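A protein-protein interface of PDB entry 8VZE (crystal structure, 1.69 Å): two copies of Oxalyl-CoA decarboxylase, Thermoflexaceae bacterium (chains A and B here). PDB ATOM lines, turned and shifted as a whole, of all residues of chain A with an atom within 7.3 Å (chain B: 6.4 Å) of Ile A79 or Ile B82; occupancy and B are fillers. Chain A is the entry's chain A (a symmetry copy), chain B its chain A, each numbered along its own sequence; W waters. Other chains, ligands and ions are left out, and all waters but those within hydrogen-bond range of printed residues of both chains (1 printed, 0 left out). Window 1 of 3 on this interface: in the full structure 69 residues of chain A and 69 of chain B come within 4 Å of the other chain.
Ile A79 touches Ala B83, and with the chains exchanged Ala A83 touches Ile B79.
Ile A79 touches Tyr B124, and with the chains exchanged Tyr A124 touches Ile B79.
His A80 touches Ala B83, and with the chains exchanged Ala A83 touches His B80.
Ser A120 touches Tyr B124, and with the chains exchanged Tyr A124 touches Ser B120.
13 positions are printed for both chains.
OH of Tyr B55 is in hydrogen-bond range of NE2 of His A80 (2.6 Å).
The side-chain hydroxyl (OG) of Ser B120 is in hydrogen-bond range of the side-chain hydroxyl (OH) of Tyr A124 (2.8 Å).
The side-chain hydroxyl of Tyr B124 is in hydrogen-bond range of the side-chain hydroxyl of Ser A120.
A ring nitrogen (ND1) of His B80 sits close to the side-chain amide nitrogen (NE2) of Gln A51.
Pro A76 touches Phe B413 (N to CE2, 3.5 Å).
Ile B82 touches Ile A79 (CG2 to CG2, 3.998 Å).
CG2 of Ile A79 touches CA of Ala B83 (3.8 Å).
Ala B86 touches Ile A79.
CZ of Phe B413 touches CD1 of Ile A79, at 3.7 Å.
His A80 touches Ala B83 (CD2 to CB, 3.7 Å).
CG2 of Ile B79 touches CG2 of Ile A82, at 3.998 Å.
Ala A83 touches Ile B79 (CA to CG2, 3.8 Å).
CD2 of His B80 touches CB of Ala A83 (3.7 Å).
Tyr B124 touches Pro A116 (OH to CD, 3.7 Å).
The side-chain amide oxygen (OE1) of Gln A117 lies within hydrogen-bond range of the backbone NH (N) of Gly A75.
OE1 of Glu A50 is in hydrogen-bond range of ND1 of His A80 (2.9 Å).
O of Pro A116 is in hydrogen-bond range of OG of Ser A120, 2.8 Å away.
OG of Ser A54 lies within hydrogen-bond range of O of Gln A51, 2.9 Å away.
Printed residues of chain B within 4 Å of Ile A79: Ile B82, Ala B83, Ala B86, Tyr B124 and Phe B413.
Printed residues of chain B within 4 Å of Ala A83: Ile B79 (3.8 Å) and His B80 (3.7 Å).
Of the printed residues of chain B, Gln A51 touches His B80.
Of the printed residues of chain A, Tyr B55 touches His A80 (2.6 Å).
Leu A97 touches none of the printed residues of chain B.
Asn B87 touches none of the printed residues of chain A.
The nearest printed residue of chain B that does not touch Ile A79 is Ile B79 (5.2 Å).
The nearest printed residue of chain A that does not touch Tyr B55 is Pro A76 (4.2 Å).
Of the 22 printed residues of chain A, 11 touch a printed residue of chain B.
Printed residues of chain A that touch a printed residue of chain B: Gln A51, Gly A75, Pro A76, Ile A79, His A80, Ile A82, Ala A83, Ala A115, Pro A116, Ser A120 and Tyr A124.
Hydrophobic or aromatic side chains of chain A within 4 Å of the printed part of chain B: Pro A76, Ile A79, His A80, Ile A82, Ala A83, Ala A115, Pro A116 and Tyr A124.
Of the 19 printed residues of chain B, 9 touch a printed residue of chain A.
Hydrophobic or aromatic side chains of chain B that line the printed part of chain A: Tyr B55, Ile B79, His B80, Ile B82, Ala B83, Ala B86, Tyr B124 and Phe B413.
Among the printed residues, 18 pairs touch across the chains.
Among the printed residues, no Asp or Glu carboxylate lies within 4 Å of a Lys or Arg side-chain nitrogen of the other chain.
Water W1 lies within hydrogen-bond range of the backbone carbonyl oxygen (O) of Ile A79 and the backbone carbonyl oxygen (O) of Ile B79.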
ATOM      1  N   GLU A  50       2.299   9.720   1.431  1.00  0.00           N
ATOM      2  CA  GLU A  50       1.964   8.424   2.017  1.00  0.00           C
ATOM      3  C   GLU A  50       2.143   7.291   1.025  1.00  0.00           C
ATOM      4  O   GLU A  50       2.295   6.142   1.440  1.00  0.00           O
ATOM      5  CB  GLU A  50       0.515   8.384   2.506  1.00  0.00           C
ATOM      6  CG  GLU A  50       0.171   9.370   3.594  1.00  0.00           C
ATOM      7  CD  GLU A  50      -0.312  10.680   3.033  1.00  0.00           C
ATOM      8  OE1 GLU A  50      -0.234  10.916   1.804  1.00  0.00           O
ATOM      9  OE2 GLU A  50      -0.756  11.475   3.865  1.00  0.00           O
ATOM     10  N   GLN A  51       2.074   7.584  -0.276  1.00  0.00           N
ATOM     11  CA  GLN A  51       2.309   6.533  -1.256  1.00  0.00           C
ATOM     12  C   GLN A  51       3.664   5.868  -1.020  1.00  0.00           C
ATOM     13  O   GLN A  51       3.762   4.644  -0.859  1.00  0.00           O
ATOM     14  CB  GLN A  51       2.223   7.132  -2.661  1.00  0.00           C
ATOM     15  CG  GLN A  51       2.288   6.109  -3.753  1.00  0.00           C
ATOM     16  CD  GLN A  51       2.444   6.773  -5.083  1.00  0.00           C
ATOM     17  OE1 GLN A  51       3.542   6.795  -5.627  1.00  0.00           O
ATOM     18  NE2 GLN A  51       1.363   7.362  -5.596  1.00  0.00           N
ATOM     19  N   SER A  54       3.835   3.932   2.268  1.00  0.00           N
ATOM     20  CA  SER A  54       3.157   2.645   2.338  1.00  0.00           C
ATOM     21  C   SER A  54       3.958   1.564   1.631  1.00  0.00           C
ATOM     22  O   SER A  54       3.886   0.392   2.011  1.00  0.00           O
ATOM     23  CB  SER A  54       1.730   2.745   1.788  1.00  0.00           C
ATOM     24  OG  SER A  54       1.721   3.009   0.384  1.00  0.00           O
ATOM     25  N   ALA A  72      -1.610   6.775   8.302  1.00  0.00           N
ATOM     26  CA  ALA A  72      -2.181   7.760   7.382  1.00  0.00           C
ATOM     27  C   ALA A  72      -3.388   8.443   8.024  1.00  0.00           C
ATOM     28  O   ALA A  72      -4.113   7.840   8.823  1.00  0.00           O
ATOM     29  CB  ALA A  72      -2.580   7.077   6.061  1.00  0.00           C
ATOM     30  N   VAL A  73      -3.593   9.716   7.675  1.00  0.00           N
ATOM     31  CA  VAL A  73      -4.791  10.450   8.096  1.00  0.00           C
ATOM     32  C   VAL A  73      -6.030   9.886   7.408  1.00  0.00           C
ATOM     33  O   VAL A  73      -5.940   9.051   6.501  1.00  0.00           O
ATOM     34  CB  VAL A  73      -4.675  11.969   7.822  1.00  0.00           C
ATOM     35  CG1 VAL A  73      -3.448  12.529   8.504  1.00  0.00           C
ATOM     36  CG2 VAL A  73      -4.603  12.304   6.319  1.00  0.00           C
ATOM     37  N   SER A  74      -7.198  10.380   7.819  1.00  0.00           N
ATOM     38  CA  SER A  74      -8.471  10.043   7.197  1.00  0.00           C
ATOM     39  C   SER A  74      -8.508  10.386   5.692  1.00  0.00           C
ATOM     40  O   SER A  74      -7.705  11.165   5.160  1.00  0.00           O
ATOM     41  CB  SER A  74      -9.615  10.782   7.924  1.00  0.00           C
ATOM     42  OG  SER A  74      -9.190  12.079   8.341  1.00  0.00           O
ATOM     43  N   GLY A  75      -9.457   9.777   5.001  1.00  0.00           N
ATOM     44  CA  GLY A  75      -9.740  10.185   3.635  1.00  0.00           C
ATOM     45  C   GLY A  75      -8.563  10.027   2.683  1.00  0.00           C
ATOM     46  O   GLY A  75      -8.064   8.919   2.447  1.00  0.00           O
ATOM     47  N   PRO A  76      -8.100  11.141   2.101  1.00  0.00           N
ATOM     48  CA  PRO A  76      -7.058  11.022   1.069  1.00  0.00           C
ATOM     49  C   PRO A  76      -5.742  10.461   1.604  1.00  0.00           C
ATOM     50  O   PRO A  76      -5.005   9.839   0.836  1.00  0.00           O
ATOM     51  CB  PRO A  76      -6.896  12.467   0.557  1.00  0.00           C
ATOM     52  CG  PRO A  76      -7.290  13.343   1.761  1.00  0.00           C
ATOM     53  CD  PRO A  76      -8.409  12.547   2.439  1.00  0.00           C
ATOM     54  N   GLY A  77      -5.426  10.644   2.889  1.00  0.00           N
ATOM     55  CA  GLY A  77      -4.216  10.020   3.425  1.00  0.00           C
ATOM     56  C   GLY A  77      -4.249   8.507   3.293  1.00  0.00           C
ATOM     57  O   GLY A  77      -3.328   7.896   2.743  1.00  0.00           O
ATOM     58  N   MET A  78      -5.346   7.897   3.749  1.00  0.00           N
ATOM     59  CA  MET A  78      -5.520   6.447   3.660  1.00  0.00           C
ATOM     60  C   MET A  78      -5.533   5.991   2.205  1.00  0.00           C
ATOM     61  O   MET A  78      -4.939   4.956   1.862  1.00  0.00           O
ATOM     62  CB  MET A  78      -6.829   6.063   4.362  1.00  0.00           C
ATOM     63  CG  MET A  78      -7.191   4.572   4.316  1.00  0.00           C
ATOM     64  SD  MET A  78      -8.144   4.134   2.831  1.00  0.00           S
ATOM     65  CE  MET A  78      -7.917   2.354   2.907  1.00  0.00           C
ATOM     66  N   ILE A  79      -6.181   6.770   1.329  1.00  0.00           N
ATOM     67  CA  ILE A  79      -6.298   6.363  -0.072  1.00  0.00           C
ATOM     68  C   ILE A  79      -4.929   6.389  -0.744  1.00  0.00           C
ATOM     69  O   ILE A  79      -4.601   5.509  -1.538  1.00  0.00           O
ATOM     70  CB  ILE A  79      -7.327   7.253  -0.796  1.00  0.00           C
ATOM     71  CG1 ILE A  79      -8.757   6.937  -0.288  1.00  0.00           C
ATOM     72  CG2 ILE A  79      -7.270   7.070  -2.348  1.00  0.00           C
ATOM     73  CD1 ILE A  79      -9.760   8.028  -0.566  1.00  0.00           C
ATOM     74  N   HIS A  80      -4.108   7.394  -0.442  1.00  0.00           N
ATOM     75  CA  HIS A  80      -2.721   7.367  -0.920  1.00  0.00           C
ATOM     76  C   HIS A  80      -1.998   6.075  -0.506  1.00  0.00           C
ATOM     77  O   HIS A  80      -1.172   5.544  -1.275  1.00  0.00           O
ATOM     78  CB  HIS A  80      -1.946   8.582  -0.401  1.00  0.00           C
ATOM     79  CG  HIS A  80      -2.358   9.888  -1.015  1.00  0.00           C
ATOM     80  ND1 HIS A  80      -1.763  11.081  -0.664  1.00  0.00           N
ATOM     81  CD2 HIS A  80      -3.300  10.196  -1.938  1.00  0.00           C
ATOM     82  CE1 HIS A  80      -2.324  12.074  -1.340  1.00  0.00           C
ATOM     83  NE2 HIS A  80      -3.267  11.565  -2.116  1.00  0.00           N
ATOM     84  N   GLY A  81      -2.299   5.558   0.705  1.00  0.00           N
ATOM     85  CA  GLY A  81      -1.658   4.362   1.237  1.00  0.00           C
ATOM     86  C   GLY A  81      -2.173   3.043   0.677  1.00  0.00           C
ATOM     87  O   GLY A  81      -1.575   1.993   0.946  1.00  0.00           O
ATOM     88  N   ILE A  82      -3.262   3.065  -0.086  1.00  0.00           N
ATOM     89  CA  ILE A  82      -3.751   1.846  -0.735  1.00  0.00           C
ATOM     90  C   ILE A  82      -2.694   1.309  -1.687  1.00  0.00           C
ATOM     91  O   ILE A  82      -2.608   0.092  -1.916  1.00  0.00           O
ATOM     92  CB  ILE A  82      -5.090   2.123  -1.445  1.00  0.00           C
ATOM     93  CG1 ILE A  82      -6.131   2.468  -0.382  1.00  0.00           C
ATOM     94  CG2 ILE A  82      -5.556   0.900  -2.261  1.00  0.00           C
ATOM     95  CD1 ILE A  82      -7.469   2.963  -0.978  1.00  0.00           C
ATOM     96  N   ALA A  83      -1.879   2.205  -2.262  1.00  0.00           N
ATOM     97  CA  ALA A  83      -0.778   1.769  -3.123  1.00  0.00           C
ATOM     98  C   ALA A  83       0.058   0.692  -2.453  1.00  0.00           C
ATOM     99  O   ALA A  83       0.344  -0.354  -3.047  1.00  0.00           O
ATOM    100  CB  ALA A  83       0.120   2.958  -3.474  1.00  0.00           C
ATOM    101  N   GLY A  84       0.483   0.947  -1.210  1.00  0.00           N
ATOM    102  CA  GLY A  84       1.273  -0.036  -0.481  1.00  0.00           C
ATOM    103  C   GLY A  84       0.505  -1.281  -0.087  1.00  0.00           C
ATOM    104  O   GLY A  84       1.078  -2.375  -0.054  1.00  0.00           O
ATOM    105  N   LEU A  97      -1.683  -1.009   7.181  1.00  0.00           N
ATOM    106  CA  LEU A  97      -2.014   0.401   7.007  1.00  0.00           C
ATOM    107  C   LEU A  97      -2.968   0.746   8.130  1.00  0.00           C
ATOM    108  O   LEU A  97      -4.001   0.075   8.282  1.00  0.00           O
ATOM    109  CB  LEU A  97      -2.666   0.649   5.643  1.00  0.00           C
ATOM    110  CG  LEU A  97      -3.176   2.070   5.367  1.00  0.00           C
ATOM    111  CD1 LEU A  97      -1.980   3.045   5.388  1.00  0.00           C
ATOM    112  CD2 LEU A  97      -3.891   2.100   3.989  1.00  0.00           C
ATOM    113  N   ALA A 115     -15.079   8.899   4.420  1.00  0.00           N
ATOM    114  CA  ALA A 115     -14.811   8.104   3.222  1.00  0.00           C
ATOM    115  C   ALA A 115     -15.021   6.634   3.546  1.00  0.00           C
ATOM    116  O   ALA A 115     -14.829   6.228   4.698  1.00  0.00           O
ATOM    117  CB  ALA A 115     -13.374   8.320   2.724  1.00  0.00           C
ATOM    118  N   PRO A 116     -15.395   5.817   2.560  1.00  0.00           N
ATOM    119  CA  PRO A 116     -15.577   4.358   2.745  1.00  0.00           C
ATOM    120  C   PRO A 116     -14.237   3.632   2.732  1.00  0.00           C
ATOM    121  O   PRO A 116     -13.873   2.936   1.774  1.00  0.00           O
ATOM    122  CB  PRO A 116     -16.446   3.986   1.536  1.00  0.00           C
ATOM    123  CG  PRO A 116     -16.004   4.949   0.452  1.00  0.00           C
ATOM    124  CD  PRO A 116     -15.701   6.255   1.180  1.00  0.00           C
ATOM    125  N   GLN A 117     -13.455   3.817   3.793  1.00  0.00           N
ATOM    126  CA  GLN A 117     -12.062   3.391   3.748  1.00  0.00           C
ATOM    127  C   GLN A 117     -11.938   1.873   3.833  1.00  0.00           C
ATOM    128  O   GLN A 117     -11.092   1.283   3.153  1.00  0.00           O
ATOM    129  CB  GLN A 117     -11.267   4.091   4.859  1.00  0.00           C
ATOM    130  CG  GLN A 117     -11.213   5.589   4.569  1.00  0.00           C
ATOM    131  CD  GLN A 117     -10.667   6.409   5.731  1.00  0.00           C
ATOM    132  OE1 GLN A 117     -10.993   7.595   5.847  1.00  0.00           O
ATOM    133  NE2 GLN A 117      -9.842   5.793   6.589  1.00  0.00           N
ATOM    134  N   SER A 120     -12.441   0.527   0.491  1.00  0.00           N
ATOM    135  CA  SER A 120     -11.369   0.863  -0.450  1.00  0.00           C
ATOM    136  C   SER A 120     -10.174  -0.050  -0.264  1.00  0.00           C
ATOM    137  O   SER A 120      -9.483  -0.387  -1.237  1.00  0.00           O
ATOM    138  CB  SER A 120     -10.951   2.322  -0.272  1.00  0.00           C
ATOM    139  OG  SER A 120     -12.094   3.168  -0.342  1.00  0.00           O
ATOM    140  N   TYR A 124      -7.383  -5.704  -1.377  1.00  0.00           N
ATOM    141  CA  TYR A 124      -5.946  -5.947  -1.252  1.00  0.00           C
ATOM    142  C   TYR A 124      -5.562  -6.513   0.097  1.00  0.00           C
ATOM    143  O   TYR A 124      -4.363  -6.774   0.327  1.00  0.00           O
ATOM    144  CB  TYR A 124      -5.158  -4.637  -1.532  1.00  0.00           C
ATOM    145  CG  TYR A 124      -5.446  -4.172  -2.925  1.00  0.00           C
ATOM    146  CD1 TYR A 124      -5.037  -4.924  -4.007  1.00  0.00           C
ATOM    147  CD2 TYR A 124      -6.187  -3.012  -3.169  1.00  0.00           C
ATOM    148  CE1 TYR A 124      -5.340  -4.538  -5.306  1.00  0.00           C
ATOM    149  CE2 TYR A 124      -6.517  -2.636  -4.477  1.00  0.00           C
ATOM    150  CZ  TYR A 124      -6.092  -3.409  -5.530  1.00  0.00           C
ATOM    151  OH  TYR A 124      -6.394  -3.073  -6.843  1.00  0.00           O
ATOM    152  N   SER B  54      -4.002  12.634 -11.381  1.00  0.00           N
ATOM    153  CA  SER B  54      -5.427  12.369 -11.234  1.00  0.00           C
ATOM    154  C   SER B  54      -6.130  13.522 -10.537  1.00  0.00           C
ATOM    155  O   SER B  54      -7.313  13.767 -10.787  1.00  0.00           O
ATOM    156  CB  SER B  54      -5.665  11.039 -10.512  1.00  0.00           C
ATOM    157  OG  SER B  54      -5.231  11.088  -9.152  1.00  0.00           O
ATOM    158  N   TYR B  55      -5.413  14.270  -9.689  1.00  0.00           N
ATOM    159  CA  TYR B  55      -5.991  15.490  -9.126  1.00  0.00           C
ATOM    160  C   TYR B  55      -6.144  16.569 -10.200  1.00  0.00           C
ATOM    161  O   TYR B  55      -7.122  17.341 -10.194  1.00  0.00           O
ATOM    162  CB  TYR B  55      -5.101  15.990  -7.984  1.00  0.00           C
ATOM    163  CG  TYR B  55      -5.117  15.132  -6.751  1.00  0.00           C
ATOM    164  CD1 TYR B  55      -6.314  14.672  -6.235  1.00  0.00           C
ATOM    165  CD2 TYR B  55      -3.932  14.771  -6.097  1.00  0.00           C
ATOM    166  CE1 TYR B  55      -6.343  13.874  -5.070  1.00  0.00           C
ATOM    167  CE2 TYR B  55      -3.944  13.971  -4.923  1.00  0.00           C
ATOM    168  CZ  TYR B  55      -5.155  13.543  -4.421  1.00  0.00           C
ATOM    169  OH  TYR B  55      -5.226  12.767  -3.284  1.00  0.00           O
ATOM    170  N   GLY B  77      -0.355   1.777 -11.422  1.00  0.00           N
ATOM    171  CA  GLY B  77      -0.673   3.059 -12.051  1.00  0.00           C
ATOM    172  C   GLY B  77      -2.101   3.493 -11.768  1.00  0.00           C
ATOM    173  O   GLY B  77      -2.346   4.604 -11.288  1.00  0.00           O
ATOM    174  N   MET B  78      -3.053   2.590 -12.012  1.00  0.00           N
ATOM    175  CA  MET B  78      -4.468   2.867 -11.759  1.00  0.00           C
ATOM    176  C   MET B  78      -4.711   3.133 -10.277  1.00  0.00           C
ATOM    177  O   MET B  78      -5.479   4.040  -9.917  1.00  0.00           O
ATOM    178  CB  MET B  78      -5.299   1.670 -12.241  1.00  0.00           C
ATOM    179  CG  MET B  78      -6.811   1.776 -12.001  1.00  0.00           C
ATOM    180  SD  MET B  78      -7.302   1.149 -10.367  1.00  0.00           S
ATOM    181  CE  MET B  78      -8.936   1.889 -10.297  1.00  0.00           C
ATOM    182  N   ILE B  79      -4.041   2.371  -9.404  1.00  0.00           N
ATOM    183  CA  ILE B  79      -4.274   2.519  -7.967  1.00  0.00           C
ATOM    184  C   ILE B  79      -3.770   3.877  -7.488  1.00  0.00           C
ATOM    185  O   ILE B  79      -4.407   4.528  -6.663  1.00  0.00           O
ATOM    186  CB  ILE B  79      -3.627   1.347  -7.204  1.00  0.00           C
ATOM    187  CG1 ILE B  79      -4.402   0.034  -7.484  1.00  0.00           C
ATOM    188  CG2 ILE B  79      -3.578   1.608  -5.663  1.00  0.00           C
ATOM    189  CD1 ILE B  79      -3.616  -1.217  -7.183  1.00  0.00           C
ATOM    190  N   HIS B  80      -2.622   4.326  -7.994  1.00  0.00           N
ATOM    191  CA  HIS B  80      -2.188   5.698  -7.704  1.00  0.00           C
ATOM    192  C   HIS B  80      -3.263   6.729  -8.081  1.00  0.00           C
ATOM    193  O   HIS B  80      -3.430   7.747  -7.380  1.00  0.00           O
ATOM    194  CB  HIS B  80      -0.883   6.019  -8.437  1.00  0.00           C
ATOM    195  CG  HIS B  80       0.321   5.297  -7.905  1.00  0.00           C
ATOM    196  ND1 HIS B  80       1.576   5.471  -8.448  1.00  0.00           N
ATOM    197  CD2 HIS B  80       0.467   4.402  -6.900  1.00  0.00           C
ATOM    198  CE1 HIS B  80       2.448   4.708  -7.804  1.00  0.00           C
ATOM    199  NE2 HIS B  80       1.800   4.041  -6.863  1.00  0.00           N
ATOM    200  N   GLY B  81      -4.001   6.479  -9.185  1.00  0.00           N
ATOM    201  CA  GLY B  81      -5.024   7.393  -9.678  1.00  0.00           C
ATOM    202  C   GLY B  81      -6.348   7.354  -8.927  1.00  0.00           C
ATOM    203  O   GLY B  81      -7.210   8.208  -9.169  1.00  0.00           O
ATOM    204  N   ILE B  82      -6.537   6.388  -8.033  1.00  0.00           N
ATOM    205  CA  ILE B  82      -7.747   6.352  -7.209  1.00  0.00           C
ATOM    206  C   ILE B  82      -7.829   7.609  -6.357  1.00  0.00           C
ATOM    207  O   ILE B  82      -8.930   8.077  -6.023  1.00  0.00           O
ATOM    208  CB  ILE B  82      -7.772   5.067  -6.357  1.00  0.00           C
ATOM    209  CG1 ILE B  82      -7.882   3.872  -7.302  1.00  0.00           C
ATOM    210  CG2 ILE B  82      -8.957   5.071  -5.371  1.00  0.00           C
ATOM    211  CD1 ILE B  82      -7.715   2.513  -6.585  1.00  0.00           C
ATOM    212  N   ALA B  83      -6.669   8.171  -5.986  1.00  0.00           N
ATOM    213  CA  ALA B  83      -6.656   9.431  -5.240  1.00  0.00           C
ATOM    214  C   ALA B  83      -7.529  10.481  -5.907  1.00  0.00           C
ATOM    215  O   ALA B  83      -8.361  11.123  -5.256  1.00  0.00           O
ATOM    216  CB  ALA B  83      -5.224   9.962  -5.130  1.00  0.00           C
ATOM    217  N   GLY B  84      -7.330  10.686  -7.213  1.00  0.00           N
ATOM    218  CA  GLY B  84      -8.134  11.659  -7.941  1.00  0.00           C
ATOM    219  C   GLY B  84      -9.587  11.264  -8.105  1.00  0.00           C
ATOM    220  O   GLY B  84     -10.466  12.131  -8.107  1.00  0.00           O
ATOM    221  N   LEU B  85      -9.872   9.965  -8.211  1.00  0.00           N
ATOM    222  CA  LEU B  85     -11.270   9.528  -8.198  1.00  0.00           C
ATOM    223  C   LEU B  85     -11.958   9.983  -6.927  1.00  0.00           C
ATOM    224  O   LEU B  85     -13.068  10.543  -6.969  1.00  0.00           O
ATOM    225  CB  LEU B  85     -11.379   8.014  -8.331  1.00  0.00           C
ATOM    226  CG  LEU B  85     -11.036   7.395  -9.691  1.00  0.00           C
ATOM    227  CD1 LEU B  85     -11.188   5.888  -9.577  1.00  0.00           C
ATOM    228  CD2 LEU B  85     -11.963   7.938 -10.775  1.00  0.00           C
ATOM    229  N   ALA B  86     -11.295   9.769  -5.789  1.00  0.00           N
ATOM    230  CA  ALA B  86     -11.897  10.088  -4.502  1.00  0.00           C
ATOM    231  C   ALA B  86     -12.024  11.593  -4.324  1.00  0.00           C
ATOM    232  O   ALA B  86     -13.018  12.077  -3.777  1.00  0.00           O
ATOM    233  CB  ALA B  86     -11.060   9.481  -3.381  1.00  0.00           C
ATOM    234  N   ASN B  87     -11.051  12.355  -4.809  1.00  0.00           N
ATOM    235  CA  ASN B  87     -11.171  13.809  -4.679  1.00  0.00           C
ATOM    236  C   ASN B  87     -12.319  14.347  -5.526  1.00  0.00           C
ATOM    237  O   ASN B  87     -13.066  15.234  -5.084  1.00  0.00           O
ATOM    238  CB  ASN B  87      -9.853  14.476  -5.050  1.00  0.00           C
ATOM    239  CG  ASN B  87      -9.686  15.790  -4.374  1.00  0.00           C
ATOM    240  OD1 ASN B  87      -9.694  15.864  -3.127  1.00  0.00           O
ATOM    241  ND2 ASN B  87      -9.553  16.859  -5.171  1.00  0.00           N
ATOM    242  N   LEU B  97     -10.918   8.393 -15.010  1.00  0.00           N
ATOM    243  CA  LEU B  97      -9.651   7.674 -14.933  1.00  0.00           C
ATOM    244  C   LEU B  97      -9.745   6.555 -15.948  1.00  0.00           C
ATOM    245  O   LEU B  97     -10.697   5.760 -15.895  1.00  0.00           O
ATOM    246  CB  LEU B  97      -9.420   7.115 -13.526  1.00  0.00           C
ATOM    247  CG  LEU B  97      -8.181   6.233 -13.324  1.00  0.00           C
ATOM    248  CD1 LEU B  97      -6.917   7.074 -13.600  1.00  0.00           C
ATOM    249  CD2 LEU B  97      -8.173   5.680 -11.874  1.00  0.00           C
ATOM    250  N   GLN B 117      -9.245  -3.892 -10.579  1.00  0.00           N
ATOM    251  CA  GLN B 117      -9.246  -2.438 -10.678  1.00  0.00           C
ATOM    252  C   GLN B 117     -10.663  -1.875 -10.630  1.00  0.00           C
ATOM    253  O   GLN B 117     -10.892  -0.828 -10.014  1.00  0.00           O
ATOM    254  CB  GLN B 117      -8.503  -2.002 -11.949  1.00  0.00           C
ATOM    255  CG  GLN B 117      -7.027  -2.369 -11.817  1.00  0.00           C
ATOM    256  CD  GLN B 117      -6.246  -2.211 -13.115  1.00  0.00           C
ATOM    257  OE1 GLN B 117      -5.230  -2.886 -13.302  1.00  0.00           O
ATOM    258  NE2 GLN B 117      -6.710  -1.328 -14.011  1.00  0.00           N
ATOM    259  N   SER B 120     -11.641  -1.623  -7.135  1.00  0.00           N
ATOM    260  CA  SER B 120     -10.892  -0.613  -6.382  1.00  0.00           C
ATOM    261  C   SER B 120     -11.441   0.776  -6.634  1.00  0.00           C
ATOM    262  O   SER B 120     -11.435   1.627  -5.733  1.00  0.00           O
ATOM    263  CB  SER B 120      -9.411  -0.671  -6.756  1.00  0.00           C
ATOM    264  OG  SER B 120      -8.924  -2.001  -6.618  1.00  0.00           O
ATOM    265  N   ALA B 121     -11.915   1.027  -7.850  1.00  0.00           N
ATOM    266  CA  ALA B 121     -12.494   2.314  -8.184  1.00  0.00           C
ATOM    267  C   ALA B 121     -13.914   2.475  -7.666  1.00  0.00           C
ATOM    268  O   ALA B 121     -14.323   3.608  -7.401  1.00  0.00           O
ATOM    269  CB  ALA B 121     -12.493   2.514  -9.690  1.00  0.00           C
ATOM    270  N   TYR B 124     -15.865   5.224  -5.353  1.00  0.00           N
ATOM    271  CA  TYR B 124     -15.702   6.648  -5.643  1.00  0.00           C
ATOM    272  C   TYR B 124     -16.309   7.050  -6.969  1.00  0.00           C
ATOM    273  O   TYR B 124     -16.245   8.244  -7.329  1.00  0.00           O
ATOM    274  CB  TYR B 124     -14.197   7.032  -5.600  1.00  0.00           C
ATOM    275  CG  TYR B 124     -13.653   6.756  -4.234  1.00  0.00           C
ATOM    276  CD1 TYR B 124     -14.107   7.476  -3.147  1.00  0.00           C
ATOM    277  CD2 TYR B 124     -12.731   5.730  -4.008  1.00  0.00           C
ATOM    278  CE1 TYR B 124     -13.653   7.200  -1.863  1.00  0.00           C
ATOM    279  CE2 TYR B 124     -12.294   5.433  -2.711  1.00  0.00           C
ATOM    280  CZ  TYR B 124     -12.767   6.171  -1.653  1.00  0.00           C
ATOM    281  OH  TYR B 124     -12.360   5.912  -0.351  1.00  0.00           O
ATOM    282  N   PHE B 413     -12.430  17.457   0.454  1.00  0.00           N
ATOM    283  CA  PHE B 413     -11.721  16.311   1.031  1.00  0.00           C
ATOM    284  C   PHE B 413     -10.483  16.742   1.828  1.00  0.00           C
ATOM    285  O   PHE B 413      -9.822  15.898   2.446  1.00  0.00           O
ATOM    286  CB  PHE B 413     -11.302  15.364  -0.100  1.00  0.00           C
ATOM    287  CG  PHE B 413     -11.382  13.866   0.221  1.00  0.00           C
ATOM    288  CD1 PHE B 413     -12.279  13.327   1.147  1.00  0.00           C
ATOM    289  CD2 PHE B 413     -10.562  12.996  -0.494  1.00  0.00           C
ATOM    290  CE1 PHE B 413     -12.346  11.921   1.361  1.00  0.00           C
ATOM    291  CE2 PHE B 413     -10.620  11.624  -0.297  1.00  0.00           C
ATOM    292  CZ  PHE B 413     -11.505  11.073   0.619  1.00  0.00           C
HETATM  293  O   HOH W   1      -3.592   5.692  -4.194  1.00  0.00           O
